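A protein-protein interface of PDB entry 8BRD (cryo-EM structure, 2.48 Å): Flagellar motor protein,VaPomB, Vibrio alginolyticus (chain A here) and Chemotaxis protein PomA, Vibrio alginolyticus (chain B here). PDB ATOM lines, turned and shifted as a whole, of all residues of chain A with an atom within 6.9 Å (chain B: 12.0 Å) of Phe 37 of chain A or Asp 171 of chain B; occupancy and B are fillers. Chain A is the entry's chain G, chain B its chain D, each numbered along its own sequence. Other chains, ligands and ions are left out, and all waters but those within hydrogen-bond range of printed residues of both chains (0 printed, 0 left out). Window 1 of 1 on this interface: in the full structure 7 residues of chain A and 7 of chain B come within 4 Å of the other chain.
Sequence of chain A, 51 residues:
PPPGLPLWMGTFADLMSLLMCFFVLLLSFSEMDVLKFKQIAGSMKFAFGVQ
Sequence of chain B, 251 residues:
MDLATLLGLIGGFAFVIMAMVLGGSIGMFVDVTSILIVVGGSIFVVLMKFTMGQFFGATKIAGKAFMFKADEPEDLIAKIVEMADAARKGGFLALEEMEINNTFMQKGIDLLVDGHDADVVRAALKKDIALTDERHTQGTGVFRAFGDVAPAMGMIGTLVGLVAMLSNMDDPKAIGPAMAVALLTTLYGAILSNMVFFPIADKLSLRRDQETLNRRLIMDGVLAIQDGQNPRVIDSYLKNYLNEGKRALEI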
ATOM      1  N   MET A  32      -4.071  10.470  16.899  1.00  0.00           N
ATOM      2  CA  MET A  32      -3.636   9.885  15.641  1.00  0.00           C
ATOM      3  C   MET A  32      -2.177  10.216  15.350  1.00  0.00           C
ATOM      4  O   MET A  32      -1.717  11.338  15.582  1.00  0.00           O
ATOM      5  CB  MET A  32      -4.525  10.387  14.508  1.00  0.00           C
ATOM      6  CG  MET A  32      -4.222   9.796  13.151  1.00  0.00           C
ATOM      7  SD  MET A  32      -5.409  10.381  11.947  1.00  0.00           S
ATOM      8  CE  MET A  32      -6.777   9.322  12.382  1.00  0.00           C
ATOM      9  N   ASP A  33      -1.452   9.231  14.831  1.00  0.00           N
ATOM     10  CA  ASP A  33      -0.090   9.411  14.352  1.00  0.00           C
ATOM     11  C   ASP A  33      -0.073   9.258  12.837  1.00  0.00           C
ATOM     12  O   ASP A  33      -0.386   8.188  12.309  1.00  0.00           O
ATOM     13  CB  ASP A  33       0.850   8.395  15.005  1.00  0.00           C
ATOM     14  CG  ASP A  33       2.304   8.620  14.643  1.00  0.00           C
ATOM     15  OD1 ASP A  33       2.609   9.595  13.928  1.00  0.00           O
ATOM     16  OD2 ASP A  33       3.149   7.815  15.082  1.00  0.00           O
ATOM     17  N   VAL A  34       0.289  10.334  12.141  1.00  0.00           N
ATOM     18  CA  VAL A  34       0.179  10.352  10.685  1.00  0.00           C
ATOM     19  C   VAL A  34       1.213   9.453  10.003  1.00  0.00           C
ATOM     20  O   VAL A  34       0.935   8.906   8.929  1.00  0.00           O
ATOM     21  CB  VAL A  34       0.259  11.798  10.162  1.00  0.00           C
ATOM     22  CG1 VAL A  34       1.700  12.248   9.973  1.00  0.00           C
ATOM     23  CG2 VAL A  34      -0.516  11.928   8.862  1.00  0.00           C
ATOM     24  N   LEU A  35       2.395   9.273  10.598  1.00  0.00           N
ATOM     25  CA  LEU A  35       3.389   8.387   9.999  1.00  0.00           C
ATOM     26  C   LEU A  35       2.889   6.949   9.976  1.00  0.00           C
ATOM     27  O   LEU A  35       2.967   6.265   8.946  1.00  0.00           O
ATOM     28  CB  LEU A  35       4.709   8.489  10.761  1.00  0.00           C
ATOM     29  CG  LEU A  35       5.537   9.754  10.523  1.00  0.00           C
ATOM     30  CD1 LEU A  35       6.954   9.560  11.032  1.00  0.00           C
ATOM     31  CD2 LEU A  35       5.543  10.127   9.048  1.00  0.00           C
ATOM     32  N   LYS A  36       2.365   6.476  11.110  1.00  0.00           N
ATOM     33  CA  LYS A  36       1.743   5.159  11.149  1.00  0.00           C
ATOM     34  C   LYS A  36       0.589   5.066  10.167  1.00  0.00           C
ATOM     35  O   LYS A  36       0.369   4.006   9.576  1.00  0.00           O
ATOM     36  CB  LYS A  36       1.259   4.840  12.562  1.00  0.00           C
ATOM     37  CG  LYS A  36       2.267   4.081  13.402  1.00  0.00           C
ATOM     38  CD  LYS A  36       2.388   4.667  14.794  1.00  0.00           C
ATOM     39  CE  LYS A  36       1.168   4.337  15.637  1.00  0.00           C
ATOM     40  NZ  LYS A  36       1.547   3.836  16.987  1.00  0.00           N
ATOM     41  N   PHE A  37      -0.152   6.158   9.972  1.00  0.00           N
ATOM     42  CA  PHE A  37      -1.221   6.129   8.985  1.00  0.00           C
ATOM     43  C   PHE A  37      -0.672   5.903   7.586  1.00  0.00           C
ATOM     44  O   PHE A  37      -1.255   5.145   6.805  1.00  0.00           O
ATOM     45  CB  PHE A  37      -2.038   7.417   9.022  1.00  0.00           C
ATOM     46  CG  PHE A  37      -3.101   7.471   7.967  1.00  0.00           C
ATOM     47  CD1 PHE A  37      -4.281   6.767   8.122  1.00  0.00           C
ATOM     48  CD2 PHE A  37      -2.909   8.195   6.804  1.00  0.00           C
ATOM     49  CE1 PHE A  37      -5.256   6.802   7.150  1.00  0.00           C
ATOM     50  CE2 PHE A  37      -3.880   8.229   5.827  1.00  0.00           C
ATOM     51  CZ  PHE A  37      -5.056   7.531   6.001  1.00  0.00           C
ATOM     52  N   LYS A  38       0.442   6.553   7.243  1.00  0.00           N
ATOM     53  CA  LYS A  38       1.030   6.339   5.924  1.00  0.00           C
ATOM     54  C   LYS A  38       1.522   4.905   5.759  1.00  0.00           C
ATOM     55  O   LYS A  38       1.307   4.286   4.706  1.00  0.00           O
ATOM     56  CB  LYS A  38       2.162   7.334   5.680  1.00  0.00           C
ATOM     57  CG  LYS A  38       1.773   8.774   5.935  1.00  0.00           C
ATOM     58  CD  LYS A  38       1.215   9.427   4.685  1.00  0.00           C
ATOM     59  CE  LYS A  38       1.460  10.926   4.692  1.00  0.00           C
ATOM     60  NZ  LYS A  38       2.736  11.275   5.375  1.00  0.00           N
ATOM     61  N   GLN A  39       2.177   4.353   6.786  1.00  0.00           N
ATOM     62  CA  GLN A  39       2.624   2.962   6.694  1.00  0.00           C
ATOM     63  C   GLN A  39       1.446   2.009   6.524  1.00  0.00           C
ATOM     64  O   GLN A  39       1.492   1.092   5.696  1.00  0.00           O
ATOM     65  CB  GLN A  39       3.444   2.554   7.918  1.00  0.00           C
ATOM     66  CG  GLN A  39       4.285   3.640   8.533  1.00  0.00           C
ATOM     67  CD  GLN A  39       5.366   3.092   9.437  1.00  0.00           C
ATOM     68  OE1 GLN A  39       5.114   2.760  10.594  1.00  0.00           O
ATOM     69  NE2 GLN A  39       6.581   2.991   8.913  1.00  0.00           N
ATOM     70  N   ILE A  40       0.381   2.210   7.299  1.00  0.00           N
ATOM     71  CA  ILE A  40      -0.768   1.316   7.229  1.00  0.00           C
ATOM     72  C   ILE A  40      -1.497   1.473   5.903  1.00  0.00           C
ATOM     73  O   ILE A  40      -2.001   0.498   5.345  1.00  0.00           O
ATOM     74  CB  ILE A  40      -1.693   1.550   8.436  1.00  0.00           C
ATOM     75  CG1 ILE A  40      -0.950   1.204   9.721  1.00  0.00           C
ATOM     76  CG2 ILE A  40      -2.938   0.704   8.328  1.00  0.00           C
ATOM     77  CD1 ILE A  40      -1.746   1.435  10.954  1.00  0.00           C
ATOM     78  N   ALA A  41      -1.561   2.696   5.370  1.00  0.00           N
ATOM     79  CA  ALA A  41      -2.177   2.893   4.062  1.00  0.00           C
ATOM     80  C   ALA A  41      -1.385   2.190   2.967  1.00  0.00           C
ATOM     81  O   ALA A  41      -1.971   1.559   2.078  1.00  0.00           O
ATOM     82  CB  ALA A  41      -2.305   4.384   3.761  1.00  0.00           C
ATOM     83  N   GLY A  42      -0.054   2.287   3.017  1.00  0.00           N
ATOM     84  CA  GLY A  42       0.762   1.562   2.057  1.00  0.00           C
ATOM     85  C   GLY A  42       0.584   0.060   2.171  1.00  0.00           C
ATOM     86  O   GLY A  42       0.464  -0.645   1.165  1.00  0.00           O
ATOM     87  N   SER A  43       0.555  -0.449   3.404  1.00  0.00           N
ATOM     88  CA  SER A  43       0.321  -1.872   3.614  1.00  0.00           C
ATOM     89  C   SER A  43      -1.058  -2.293   3.121  1.00  0.00           C
ATOM     90  O   SER A  43      -1.230  -3.421   2.647  1.00  0.00           O
ATOM     91  CB  SER A  43       0.485  -2.210   5.094  1.00  0.00           C
ATOM     92  OG  SER A  43       0.232  -3.580   5.329  1.00  0.00           O
ATOM     93  N   GLY B 161     -17.407  -1.424  -0.833  1.00  0.00           N
ATOM     94  CA  GLY B 161     -17.076  -0.029  -0.595  1.00  0.00           C
ATOM     95  C   GLY B 161     -15.947   0.143   0.398  1.00  0.00           C
ATOM     96  O   GLY B 161     -15.080   1.000   0.224  1.00  0.00           O
ATOM     97  N   LEU B 162     -15.930  -0.678   1.446  1.00  0.00           N
ATOM     98  CA  LEU B 162     -14.867  -0.578   2.437  1.00  0.00           C
ATOM     99  C   LEU B 162     -13.533  -1.067   1.890  1.00  0.00           C
ATOM    100  O   LEU B 162     -12.481  -0.501   2.206  1.00  0.00           O
ATOM    101  CB  LEU B 162     -15.259  -1.352   3.686  1.00  0.00           C
ATOM    102  CG  LEU B 162     -16.357  -0.650   4.473  1.00  0.00           C
ATOM    103  CD1 LEU B 162     -16.811  -1.523   5.599  1.00  0.00           C
ATOM    104  CD2 LEU B 162     -15.870   0.690   4.995  1.00  0.00           C
ATOM    105  N   ALA B 164     -12.704  -0.826  -1.252  1.00  0.00           N
ATOM    106  CA  ALA B 164     -12.296   0.276  -2.114  1.00  0.00           C
ATOM    107  C   ALA B 164     -11.734   1.442  -1.314  1.00  0.00           C
ATOM    108  O   ALA B 164     -10.798   2.109  -1.769  1.00  0.00           O
ATOM    109  CB  ALA B 164     -13.473   0.741  -2.965  1.00  0.00           C
ATOM    110  N   MET B 165     -12.300   1.718  -0.140  1.00  0.00           N
ATOM    111  CA  MET B 165     -11.789   2.807   0.685  1.00  0.00           C
ATOM    112  C   MET B 165     -10.410   2.475   1.238  1.00  0.00           C
ATOM    113  O   MET B 165      -9.529   3.342   1.290  1.00  0.00           O
ATOM    114  CB  MET B 165     -12.767   3.108   1.818  1.00  0.00           C
ATOM    115  CG  MET B 165     -12.162   3.889   2.967  1.00  0.00           C
ATOM    116  SD  MET B 165     -13.065   3.732   4.511  1.00  0.00           S
ATOM    117  CE  MET B 165     -12.084   2.498   5.335  1.00  0.00           C
ATOM    118  N   LEU B 166     -10.202   1.226   1.657  1.00  0.00           N
ATOM    119  CA  LEU B 166      -8.903   0.814   2.170  1.00  0.00           C
ATOM    120  C   LEU B 166      -7.858   0.674   1.074  1.00  0.00           C
ATOM    121  O   LEU B 166      -6.661   0.744   1.365  1.00  0.00           O
ATOM    122  CB  LEU B 166      -9.035  -0.503   2.928  1.00  0.00           C
ATOM    123  CG  LEU B 166      -9.782  -0.392   4.251  1.00  0.00           C
ATOM    124  CD1 LEU B 166      -9.911  -1.748   4.896  1.00  0.00           C
ATOM    125  CD2 LEU B 166      -9.039   0.558   5.155  1.00  0.00           C
ATOM    126  N   SER B 167      -8.287   0.470  -0.174  1.00  0.00           N
ATOM    127  CA  SER B 167      -7.340   0.336  -1.274  1.00  0.00           C
ATOM    128  C   SER B 167      -6.576   1.629  -1.519  1.00  0.00           C
ATOM    129  O   SER B 167      -5.418   1.593  -1.950  1.00  0.00           O
ATOM    130  CB  SER B 167      -8.075  -0.094  -2.540  1.00  0.00           C
ATOM    131  OG  SER B 167      -8.776  -1.304  -2.329  1.00  0.00           O
ATOM    132  N   ASN B 168      -7.197   2.777  -1.257  1.00  0.00           N
ATOM    133  CA  ASN B 168      -6.525   4.064  -1.419  1.00  0.00           C
ATOM    134  C   ASN B 168      -7.064   5.006  -0.347  1.00  0.00           C
ATOM    135  O   ASN B 168      -8.095   5.653  -0.549  1.00  0.00           O
ATOM    136  CB  ASN B 168      -6.733   4.621  -2.822  1.00  0.00           C
ATOM    137  CG  ASN B 168      -8.175   4.534  -3.280  1.00  0.00           C
ATOM    138  OD1 ASN B 168      -8.579   3.559  -3.913  1.00  0.00           O
ATOM    139  ND2 ASN B 168      -8.958   5.556  -2.961  1.00  0.00           N
ATOM    140  N   MET B 169      -6.364   5.082   0.781  1.00  0.00           N
ATOM    141  CA  MET B 169      -6.824   5.912   1.900  1.00  0.00           C
ATOM    142  C   MET B 169      -6.427   7.368   1.677  1.00  0.00           C
ATOM    143  O   MET B 169      -7.287   8.236   1.506  1.00  0.00           O
ATOM    144  CB  MET B 169      -6.258   5.367   3.212  1.00  0.00           C
ATOM    145  CG  MET B 169      -6.728   3.962   3.544  1.00  0.00           C
ATOM    146  SD  MET B 169      -6.958   3.690   5.308  1.00  0.00           S
ATOM    147  CE  MET B 169      -5.406   2.921   5.744  1.00  0.00           C
ATOM    148  N   ASP B 170      -5.121   7.647   1.699  1.00  0.00           N
ATOM    149  CA  ASP B 170      -4.548   8.918   1.257  1.00  0.00           C
ATOM    150  C   ASP B 170      -4.971  10.065   2.176  1.00  0.00           C
ATOM    151  O   ASP B 170      -4.340  11.125   2.182  1.00  0.00           O
ATOM    152  CB  ASP B 170      -4.929   9.116  -0.231  1.00  0.00           C
ATOM    153  CG  ASP B 170      -4.728  10.544  -0.772  1.00  0.00           C
ATOM    154  OD1 ASP B 170      -5.031  11.563  -0.122  1.00  0.00           O
ATOM    155  OD2 ASP B 170      -4.366  10.635  -1.962  1.00  0.00           O
ATOM    156  N   ASP B 171      -5.941   9.826   3.051  1.00  0.00           N
ATOM    157  CA  ASP B 171      -6.468  10.877   3.911  1.00  0.00           C
ATOM    158  C   ASP B 171      -7.199  10.251   5.091  1.00  0.00           C
ATOM    159  O   ASP B 171      -8.129   9.457   4.895  1.00  0.00           O
ATOM    160  CB  ASP B 171      -7.402  11.796   3.119  1.00  0.00           C
ATOM    161  CG  ASP B 171      -7.711  13.090   3.846  1.00  0.00           C
ATOM    162  OD1 ASP B 171      -7.279  13.250   5.006  1.00  0.00           O
ATOM    163  OD2 ASP B 171      -8.386  13.957   3.252  1.00  0.00           O
ATOM    164  N   PRO B 172      -6.811  10.575   6.326  1.00  0.00           N
ATOM    165  CA  PRO B 172      -7.506   9.972   7.476  1.00  0.00           C
ATOM    166  C   PRO B 172      -8.846  10.616   7.776  1.00  0.00           C
ATOM    167  O   PRO B 172      -9.760   9.933   8.251  1.00  0.00           O
ATOM    168  CB  PRO B 172      -6.509  10.169   8.624  1.00  0.00           C
ATOM    169  CG  PRO B 172      -5.667  11.318   8.206  1.00  0.00           C
ATOM    170  CD  PRO B 172      -5.554  11.234   6.720  1.00  0.00           C
ATOM    171  N   LYS B 173      -8.996  11.916   7.522  1.00  0.00           N
ATOM    172  CA  LYS B 173     -10.263  12.583   7.784  1.00  0.00           C
ATOM    173  C   LYS B 173     -11.359  12.173   6.814  1.00  0.00           C
ATOM    174  O   LYS B 173     -12.525  12.502   7.047  1.00  0.00           O
ATOM    175  CB  LYS B 173     -10.086  14.102   7.742  1.00  0.00           C
ATOM    176  CG  LYS B 173      -9.360  14.668   8.948  1.00  0.00           C
ATOM    177  CD  LYS B 173      -9.397  16.185   8.954  1.00  0.00           C
ATOM    178  CE  LYS B 173      -8.742  16.741  10.206  1.00  0.00           C
ATOM    179  NZ  LYS B 173      -9.526  17.868  10.781  1.00  0.00           N
ATOM    180  N   ALA B 174     -11.015  11.477   5.738  1.00  0.00           N
ATOM    181  CA  ALA B 174     -11.989  10.959   4.790  1.00  0.00           C
ATOM    182  C   ALA B 174     -12.374   9.514   5.072  1.00  0.00           C
ATOM    183  O   ALA B 174     -13.157   8.940   4.310  1.00  0.00           O
ATOM    184  CB  ALA B 174     -11.449  11.084   3.363  1.00  0.00           C
ATOM    185  N   ILE B 175     -11.837   8.911   6.134  1.00  0.00           N
ATOM    186  CA  ILE B 175     -12.145   7.516   6.434  1.00  0.00           C
ATOM    187  C   ILE B 175     -13.605   7.363   6.839  1.00  0.00           C
ATOM    188  O   ILE B 175     -14.327   6.518   6.300  1.00  0.00           O
ATOM    189  CB  ILE B 175     -11.201   6.982   7.527  1.00  0.00           C
ATOM    190  CG1 ILE B 175      -9.759   6.975   7.031  1.00  0.00           C
ATOM    191  CG2 ILE B 175     -11.606   5.581   7.934  1.00  0.00           C
ATOM    192  CD1 ILE B 175      -9.520   5.997   5.920  1.00  0.00           C
ATOM    193  N   GLY B 176     -14.066   8.194   7.771  1.00  0.00           N
ATOM    194  CA  GLY B 176     -15.405   8.097   8.302  1.00  0.00           C
ATOM    195  C   GLY B 176     -16.512   8.243   7.276  1.00  0.00           C
ATOM    196  O   GLY B 176     -17.412   7.403   7.190  1.00  0.00           O
ATOM    197  N   PRO B 177     -16.485   9.325   6.488  1.00  0.00           N
ATOM    198  CA  PRO B 177     -17.502   9.475   5.433  1.00  0.00           C
ATOM    199  C   PRO B 177     -17.522   8.330   4.434  1.00  0.00           C
ATOM    200  O   PRO B 177     -18.598   7.939   3.954  1.00  0.00           O
ATOM    201  CB  PRO B 177     -17.115  10.805   4.781  1.00  0.00           C
ATOM    202  CG  PRO B 177     -16.470  11.565   5.869  1.00  0.00           C
ATOM    203  CD  PRO B 177     -15.707  10.562   6.670  1.00  0.00           C
ATOM    204  N   ALA B 178     -16.356   7.772   4.108  1.00  0.00           N
ATOM    205  CA  ALA B 178     -16.311   6.636   3.195  1.00  0.00           C
ATOM    206  C   ALA B 178     -17.034   5.431   3.782  1.00  0.00           C
ATOM    207  O   ALA B 178     -17.795   4.751   3.084  1.00  0.00           O
ATOM    208  CB  ALA B 178     -14.863   6.295   2.855  1.00  0.00           C
ATOM    209  N   MET B 179     -16.823   5.149   5.073  1.00  0.00           N
ATOM    210  CA  MET B 179     -17.538   4.041   5.698  1.00  0.00           C
ATOM    211  C   MET B 179     -19.024   4.337   5.831  1.00  0.00           C
ATOM    212  O   MET B 179     -19.849   3.425   5.767  1.00  0.00           O
ATOM    213  CB  MET B 179     -16.944   3.678   7.061  1.00  0.00           C
ATOM    214  CG  MET B 179     -15.453   3.842   7.195  1.00  0.00           C
ATOM    215  SD  MET B 179     -14.830   2.894   8.599  1.00  0.00           S
ATOM    216  CE  MET B 179     -14.345   4.187   9.725  1.00  0.00           C
ATOM    217  N   ALA B 180     -19.388   5.605   6.020  1.00  0.00           N
ATOM    218  CA  ALA B 180     -20.806   5.960   6.043  1.00  0.00           C
ATOM    219  C   ALA B 180     -21.471   5.640   4.711  1.00  0.00           C
ATOM    220  O   ALA B 180     -22.542   5.017   4.661  1.00  0.00           O
ATOM    221  CB  ALA B 180     -20.964   7.441   6.385  1.00  0.00           C
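The side-chain carboxylate (OD1) of Asp 171 of chain B sits at hydrogen-bond distance from the backbone NH (N) of Lys 173 of chain B.
Among the printed residues, pairs that only touch across the chains: Met 32 of chain A with Pro 172 of chain B (3.5 Å), Phe 37 of chain A with Met 169 of chain B (3.7 Å), Phe 37 of chain A with Asp 171 of chain B (3.6 Å), Phe 37 of chain A with Pro 172 of chain B (3.5 Å) and Ala 41 of chain A with Met 169 of chain B (3.6 Å).
No residue of chain B comes within 4 Å of Asp 33 of chain A. No residue of chain B comes within 4 Å of Leu 35 of chain A. No residue of chain B comes within 4 Å of Lys 36 of chain A. Phe 37 of chain A touches just these residues of chain B: Met 169, Asp 171 and Pro 172. Ile 40 of chain A touches none of the printed residues of chain B. Printed residues of chain A within 4 Å of Met 169 of chain B: Phe 37 (3.7 Å) and Ala 41 (3.6 Å). Asp 170 of chain B touches none of the printed residues of chain A. Of the printed residues of chain A, Pro 172 of chain B touches Met 32 and Phe 37. The nearest residue of chain A that does not touch Asp 171 of chain B is Ala 41 of chain A (6.6 Å).
Of the 12 printed residues of chain A, 3 touch a printed residue of chain B. Printed residues of chain A that touch a printed residue of chain B: Met 32, Phe 37 and Ala 41. Printed residues of chain B that touch a printed residue of chain A: Met 169, Asp 171 and Pro 172. Hydrophobic or aromatic side chains of chain B that line the printed part of chain A: Met 169 and Pro 172. Among the printed residues, 5 pairs touch across the chains. Among the printed residues, no Asp or Glu carboxylate lies within 4 Å of a Lys or Arg side-chain nitrogen of the other chain.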
